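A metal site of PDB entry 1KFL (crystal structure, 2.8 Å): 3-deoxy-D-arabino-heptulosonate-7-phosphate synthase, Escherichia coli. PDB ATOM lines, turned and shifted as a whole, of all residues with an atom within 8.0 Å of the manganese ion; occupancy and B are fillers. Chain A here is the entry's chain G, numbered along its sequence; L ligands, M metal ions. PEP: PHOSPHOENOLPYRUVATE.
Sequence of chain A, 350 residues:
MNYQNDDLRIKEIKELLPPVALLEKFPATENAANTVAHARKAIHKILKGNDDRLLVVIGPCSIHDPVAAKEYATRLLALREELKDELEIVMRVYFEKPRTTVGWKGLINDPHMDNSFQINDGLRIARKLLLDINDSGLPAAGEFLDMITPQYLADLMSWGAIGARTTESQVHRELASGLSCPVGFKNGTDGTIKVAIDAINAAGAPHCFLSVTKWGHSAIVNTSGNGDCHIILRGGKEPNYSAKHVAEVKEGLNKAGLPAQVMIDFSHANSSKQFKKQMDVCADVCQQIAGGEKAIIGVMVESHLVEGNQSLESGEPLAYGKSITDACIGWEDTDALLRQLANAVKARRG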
ATOM      1  N   GLY A  59     -14.676  25.354  14.335  1.00  0.00           N
ATOM      2  CA  GLY A  59     -14.353  26.485  15.176  1.00  0.00           C
ATOM      3  C   GLY A  59     -13.942  26.108  16.574  1.00  0.00           C
ATOM      4  O   GLY A  59     -13.974  24.925  16.919  1.00  0.00           O
ATOM      5  N   PRO A  60     -13.551  27.085  17.428  1.00  0.00           N
ATOM      6  CA  PRO A  60     -13.125  26.850  18.815  1.00  0.00           C
ATOM      7  C   PRO A  60     -14.122  26.016  19.613  1.00  0.00           C
ATOM      8  O   PRO A  60     -15.329  26.161  19.455  1.00  0.00           O
ATOM      9  CB  PRO A  60     -12.999  28.266  19.371  1.00  0.00           C
ATOM     10  CG  PRO A  60     -12.571  29.059  18.180  1.00  0.00           C
ATOM     11  CD  PRO A  60     -13.489  28.533  17.101  1.00  0.00           C
ATOM     12  N   CYS A  61     -13.607  25.151  20.488  1.00  0.00           N
ATOM     13  CA  CYS A  61     -14.468  24.319  21.326  1.00  0.00           C
ATOM     14  C   CYS A  61     -15.450  25.221  22.063  1.00  0.00           C
ATOM     15  O   CYS A  61     -16.654  24.941  22.133  1.00  0.00           O
ATOM     16  CB  CYS A  61     -13.644  23.554  22.358  1.00  0.00           C
ATOM     17  SG  CYS A  61     -14.660  22.905  23.716  1.00  0.00           S
ATOM     18  N   SER A  62     -14.913  26.295  22.637  1.00  0.00           N
ATOM     19  CA  SER A  62     -15.683  27.284  23.365  1.00  0.00           C
ATOM     20  C   SER A  62     -14.972  28.622  23.171  1.00  0.00           C
ATOM     21  O   SER A  62     -13.741  28.667  23.044  1.00  0.00           O
ATOM     22  CB  SER A  62     -15.730  26.957  24.851  1.00  0.00           C
ATOM     23  OG  SER A  62     -14.477  27.199  25.462  1.00  0.00           O
ATOM     24  N   ARG A  92     -18.092  27.672  14.374  1.00  0.00           N
ATOM     25  CA  ARG A  92     -18.601  27.069  15.604  1.00  0.00           C
ATOM     26  C   ARG A  92     -18.445  28.097  16.720  1.00  0.00           C
ATOM     27  O   ARG A  92     -17.364  28.245  17.291  1.00  0.00           O
ATOM     28  CB  ARG A  92     -17.792  25.812  15.948  1.00  0.00           C
ATOM     29  CG  ARG A  92     -18.114  25.207  17.305  1.00  0.00           C
ATOM     30  CD  ARG A  92     -17.078  24.144  17.693  1.00  0.00           C
ATOM     31  NE  ARG A  92     -17.217  23.721  19.092  1.00  0.00           N
ATOM     32  CZ  ARG A  92     -17.982  22.725  19.503  1.00  0.00           C
ATOM     33  NH1 ARG A  92     -18.698  22.018  18.628  1.00  0.00           N
ATOM     34  NH2 ARG A  92     -18.064  22.440  20.798  1.00  0.00           N
ATOM     35  N   TYR A  94     -19.477  28.547  20.136  1.00  0.00           N
ATOM     36  CA  TYR A  94     -20.042  28.014  21.369  1.00  0.00           C
ATOM     37  C   TYR A  94     -19.497  28.815  22.552  1.00  0.00           C
ATOM     38  O   TYR A  94     -18.306  29.122  22.613  1.00  0.00           O
ATOM     39  CB  TYR A  94     -19.671  26.534  21.529  1.00  0.00           C
ATOM     40  CG  TYR A  94     -20.455  25.557  20.635  1.00  0.00           C
ATOM     41  CD1 TYR A  94     -20.771  25.874  19.312  1.00  0.00           C
ATOM     42  CD2 TYR A  94     -20.812  24.288  21.111  1.00  0.00           C
ATOM     43  CE1 TYR A  94     -21.424  24.956  18.485  1.00  0.00           C
ATOM     44  CE2 TYR A  94     -21.462  23.366  20.297  1.00  0.00           C
ATOM     45  CZ  TYR A  94     -21.760  23.707  18.985  1.00  0.00           C
ATOM     46  OH  TYR A  94     -22.381  22.770  18.176  1.00  0.00           O
ATOM     47  N   GLU A  96     -20.166  27.935  25.995  1.00  0.00           N
ATOM     48  CA  GLU A  96     -19.960  27.132  27.188  1.00  0.00           C
ATOM     49  C   GLU A  96     -20.042  25.639  26.946  1.00  0.00           C
ATOM     50  O   GLU A  96     -20.775  25.175  26.075  1.00  0.00           O
ATOM     51  CB  GLU A  96     -20.997  27.515  28.256  1.00  0.00           C
ATOM     52  CG  GLU A  96     -21.747  26.317  28.827  1.00  0.00           C
ATOM     53  CD  GLU A  96     -22.741  26.698  29.901  1.00  0.00           C
ATOM     54  OE1 GLU A  96     -23.672  27.488  29.617  1.00  0.00           O
ATOM     55  OE2 GLU A  96     -22.597  26.191  31.034  1.00  0.00           O
ATOM     56  N   LYS A  97     -19.278  24.889  27.730  1.00  0.00           N
ATOM     57  CA  LYS A  97     -19.286  23.431  27.651  1.00  0.00           C
ATOM     58  C   LYS A  97     -19.835  22.873  28.964  1.00  0.00           C
ATOM     59  O   LYS A  97     -19.331  23.161  30.038  1.00  0.00           O
ATOM     60  CB  LYS A  97     -17.877  22.872  27.402  1.00  0.00           C
ATOM     61  CG  LYS A  97     -17.835  21.353  27.557  1.00  0.00           C
ATOM     62  CD  LYS A  97     -16.659  20.720  26.865  1.00  0.00           C
ATOM     63  CE  LYS A  97     -16.772  19.207  26.948  1.00  0.00           C
ATOM     64  NZ  LYS A  97     -15.734  18.495  26.169  1.00  0.00           N
ATOM     65  N   PRO A  98     -20.902  22.064  28.877  1.00  0.00           N
ATOM     66  CA  PRO A  98     -21.490  21.458  30.077  1.00  0.00           C
ATOM     67  C   PRO A  98     -20.462  20.619  30.832  1.00  0.00           C
ATOM     68  O   PRO A  98     -19.846  19.709  30.267  1.00  0.00           O
ATOM     69  CB  PRO A  98     -22.627  20.613  29.510  1.00  0.00           C
ATOM     70  CG  PRO A  98     -23.036  21.397  28.277  1.00  0.00           C
ATOM     71  CD  PRO A  98     -21.700  21.771  27.680  1.00  0.00           C
ATOM     72  N   GLU A 143     -24.852  26.244  20.039  1.00  0.00           N
ATOM     73  CA  GLU A 143     -25.504  25.134  20.723  1.00  0.00           C
ATOM     74  C   GLU A 143     -26.522  25.738  21.661  1.00  0.00           C
ATOM     75  O   GLU A 143     -26.343  26.855  22.142  1.00  0.00           O
ATOM     76  CB  GLU A 143     -24.465  24.323  21.507  1.00  0.00           C
ATOM     77  CG  GLU A 143     -25.035  23.236  22.394  1.00  0.00           C
ATOM     78  CD  GLU A 143     -23.947  22.405  23.048  1.00  0.00           C
ATOM     79  OE1 GLU A 143     -22.973  23.006  23.564  1.00  0.00           O
ATOM     80  OE2 GLU A 143     -24.076  21.158  23.052  1.00  0.00           O
ATOM     81  N   LYS A 186     -26.942  15.170  18.502  1.00  0.00           N
ATOM     82  CA  LYS A 186     -25.796  14.291  18.661  1.00  0.00           C
ATOM     83  C   LYS A 186     -26.231  12.948  19.227  1.00  0.00           C
ATOM     84  O   LYS A 186     -27.220  12.879  19.961  1.00  0.00           O
ATOM     85  CB  LYS A 186     -24.769  14.921  19.599  1.00  0.00           C
ATOM     86  CG  LYS A 186     -24.081  16.139  19.031  1.00  0.00           C
ATOM     87  CD  LYS A 186     -22.748  16.378  19.707  1.00  0.00           C
ATOM     88  CE  LYS A 186     -21.788  17.066  18.758  1.00  0.00           C
ATOM     89  NZ  LYS A 186     -20.376  17.006  19.248  1.00  0.00           N
ATOM     90  N   ASP A 265     -18.617  14.290  13.547  1.00  0.00           N
ATOM     91  CA  ASP A 265     -17.822  15.145  14.423  1.00  0.00           C
ATOM     92  C   ASP A 265     -16.418  14.533  14.574  1.00  0.00           C
ATOM     93  O   ASP A 265     -16.246  13.511  15.229  1.00  0.00           O
ATOM     94  CB  ASP A 265     -18.522  15.258  15.782  1.00  0.00           C
ATOM     95  CG  ASP A 265     -17.773  16.134  16.757  1.00  0.00           C
ATOM     96  OD1 ASP A 265     -16.936  16.951  16.289  1.00  0.00           O
ATOM     97  OD2 ASP A 265     -18.027  16.015  17.973  1.00  0.00           O
ATOM     98  N   SER A 267     -14.041  15.593  16.252  1.00  0.00           N
ATOM     99  CA  SER A 267     -13.531  15.774  17.601  1.00  0.00           C
ATOM    100  C   SER A 267     -14.256  14.911  18.643  1.00  0.00           C
ATOM    101  O   SER A 267     -14.954  13.957  18.306  1.00  0.00           O
ATOM    102  CB  SER A 267     -13.619  17.267  17.977  1.00  0.00           C
ATOM    103  OG  SER A 267     -12.854  17.556  19.118  1.00  0.00           O
ATOM    104  N   HIS A 268     -14.062  15.260  19.915  1.00  0.00           N
ATOM    105  CA  HIS A 268     -14.667  14.551  21.048  1.00  0.00           C
ATOM    106  C   HIS A 268     -14.442  13.041  20.995  1.00  0.00           C
ATOM    107  O   HIS A 268     -13.337  12.604  20.719  1.00  0.00           O
ATOM    108  CB  HIS A 268     -16.162  14.872  21.141  1.00  0.00           C
ATOM    109  CG  HIS A 268     -16.446  16.341  21.195  1.00  0.00           C
ATOM    110  ND1 HIS A 268     -16.585  17.113  20.069  1.00  0.00           N
ATOM    111  CD2 HIS A 268     -16.505  17.193  22.254  1.00  0.00           C
ATOM    112  CE1 HIS A 268     -16.718  18.385  20.421  1.00  0.00           C
ATOM    113  NE2 HIS A 268     -16.674  18.454  21.734  1.00  0.00           N
ATOM    114  N   MET A 300     -17.873  18.237  11.614  1.00  0.00           N
ATOM    115  CA  MET A 300     -17.670  19.193  12.689  1.00  0.00           C
ATOM    116  C   MET A 300     -16.234  19.080  13.180  1.00  0.00           C
ATOM    117  O   MET A 300     -15.776  17.990  13.520  1.00  0.00           O
ATOM    118  CB  MET A 300     -18.629  18.909  13.826  1.00  0.00           C
ATOM    119  CG  MET A 300     -18.657  19.971  14.884  1.00  0.00           C
ATOM    120  SD  MET A 300     -20.045  19.617  16.163  1.00  0.00           S
ATOM    121  CE  MET A 300     -18.947  19.070  17.637  1.00  0.00           C
ATOM    122  N   GLU A 302     -13.168  20.868  15.784  1.00  0.00           N
ATOM    123  CA  GLU A 302     -12.761  21.810  16.819  1.00  0.00           C
ATOM    124  C   GLU A 302     -11.373  22.331  16.477  1.00  0.00           C
ATOM    125  O   GLU A 302     -10.401  21.581  16.524  1.00  0.00           O
ATOM    126  CB  GLU A 302     -12.743  21.146  18.201  1.00  0.00           C
ATOM    127  CG  GLU A 302     -14.120  20.699  18.670  1.00  0.00           C
ATOM    128  CD  GLU A 302     -14.170  20.432  20.161  1.00  0.00           C
ATOM    129  OE1 GLU A 302     -13.385  19.582  20.637  1.00  0.00           O
ATOM    130  OE2 GLU A 302     -14.999  21.058  20.855  1.00  0.00           O
ATOM    131  N   SER A 323      -7.657  27.425  23.011  1.00  0.00           N
ATOM    132  CA  SER A 323      -8.792  26.916  23.788  1.00  0.00           C
ATOM    133  C   SER A 323      -8.515  26.761  25.284  1.00  0.00           C
ATOM    134  O   SER A 323      -7.387  26.469  25.684  1.00  0.00           O
ATOM    135  CB  SER A 323      -9.233  25.546  23.221  1.00  0.00           C
ATOM    136  OG  SER A 323     -10.334  25.022  23.949  1.00  0.00           O
ATOM    137  N   THR A 325     -10.830  24.916  27.026  1.00  0.00           N
ATOM    138  CA  THR A 325     -11.712  23.771  27.278  1.00  0.00           C
ATOM    139  C   THR A 325     -11.076  22.591  26.540  1.00  0.00           C
ATOM    140  O   THR A 325      -9.951  22.198  26.856  1.00  0.00           O
ATOM    141  CB  THR A 325     -13.150  24.016  26.762  1.00  0.00           C
ATOM    142  OG1 THR A 325     -13.112  24.750  25.526  1.00  0.00           O
ATOM    143  CG2 THR A 325     -13.964  24.804  27.782  1.00  0.00           C
ATOM    144  N   ASP A 326     -11.778  22.023  25.555  1.00  0.00           N
ATOM    145  CA  ASP A 326     -11.227  20.904  24.778  1.00  0.00           C
ATOM    146  C   ASP A 326     -10.081  21.360  23.876  1.00  0.00           C
ATOM    147  O   ASP A 326     -10.045  22.519  23.440  1.00  0.00           O
ATOM    148  CB  ASP A 326     -12.301  20.243  23.908  1.00  0.00           C
ATOM    149  CG  ASP A 326     -13.408  19.602  24.722  1.00  0.00           C
ATOM    150  OD1 ASP A 326     -13.176  19.340  25.921  1.00  0.00           O
ATOM    151  OD2 ASP A 326     -14.492  19.344  24.147  1.00  0.00           O
ATOM    152  N   ALA A 327      -9.169  20.436  23.593  1.00  0.00           N
ATOM    153  CA  ALA A 327      -8.026  20.734  22.733  1.00  0.00           C
ATOM    154  C   ALA A 327      -8.492  20.818  21.283  1.00  0.00           C
ATOM    155  O   ALA A 327      -9.316  20.015  20.846  1.00  0.00           O
ATOM    156  CB  ALA A 327      -6.962  19.654  22.882  1.00  0.00           C
ATOM    157  N   CYS A 328      -7.973  21.809  20.559  1.00  0.00           N
ATOM    158  CA  CYS A 328      -8.326  22.029  19.160  1.00  0.00           C
ATOM    159  C   CYS A 328      -7.076  21.953  18.288  1.00  0.00           C
ATOM    160  O   CYS A 328      -5.962  22.177  18.762  1.00  0.00           O
ATOM    161  CB  CYS A 328      -8.969  23.414  18.988  1.00  0.00           C
ATOM    162  SG  CYS A 328     -10.331  23.815  20.137  1.00  0.00           S
HETATM  163  C1  PEP L   1     -19.886  15.947  22.939  1.00  0.00           C
HETATM  164  O1  PEP L   1     -20.301  15.104  23.817  1.00  0.00           O
HETATM  165  O2' PEP L   1     -19.322  15.607  21.921  1.00  0.00           O
HETATM  166  C2  PEP L   1     -20.143  17.398  23.305  1.00  0.00           C
HETATM  167  C3  PEP L   1     -20.753  17.917  24.411  1.00  0.00           C
HETATM  168  O2  PEP L   1     -19.692  18.313  22.344  1.00  0.00           O
HETATM  169  P   PEP L   1     -20.436  19.624  21.823  1.00  0.00           P
HETATM  170  O1P PEP L   1     -19.995  19.796  20.342  1.00  0.00           O
HETATM  171  O2P PEP L   1     -19.937  20.713  22.743  1.00  0.00           O
HETATM  172  O3P PEP L   1     -21.903  19.373  21.828  1.00  0.00           O
HETATM  173 MN    MN M   1     -15.647  20.336  22.771  1.00  0.00          MN
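The manganese ion is bound by OD2 of Asp 326 (2.1 Å), OE2 of Glu 302 (2.1 Å) and NE2 of His 268 (2.4 Å). Slightly farther from the manganese ion lies SG of Cys 61 (2.9 Å).
Residues that only touch the manganese ion: Arg 92 and Lys 97. Within 4 Å of the manganese ion: Cys 61, Arg 92, Lys 97, His 268, Glu 302 and Asp 326.
The backbone NH (N) of Asp 326 is in hydrogen-bond range of the side-chain sulfur (SG) of Cys 61. The side-chain carboxylate of Asp 326 lies within salt-bridge range of the side-chain amino group of Lys 97. NH2 of Arg 92 sits close to OE2 of Glu 302 (3.4 Å). The guanidinium group (NH2) of Arg 92 sits at hydrogen-bond distance from the backbone carbonyl oxygen (O) of Cys 61, 3.2 Å away. The side-chain sulfur of Cys 61 is in hydrogen-bond range of the side-chain hydroxyl of Thr 325 (3.0 Å). SG of Cys 328 sits at hydrogen-bond distance from N of Cys 61 (3.6 Å). The side-chain sulfur (SD) of Met 300 sits close to the guanidinium group (NH1) of Arg 92. The guanidinium group of Arg 92 lies within hydrogen-bond range of the backbone carbonyl oxygen of Pro 60, 3.1 Å away.
NE2 of His 268 lies close to O2 of the ligand (3.1 Å). O1P of the ligand lies within salt-bridge range of NH1 of Arg 92 (3.1 Å). An oxygen (O1P) of the ligand is in salt-bridge range of the side-chain amino group (NZ) of Lys 186. The side-chain carboxylate of Glu 143 lies close to an oxygen (O3P) of the ligand, 3.1 Å away.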
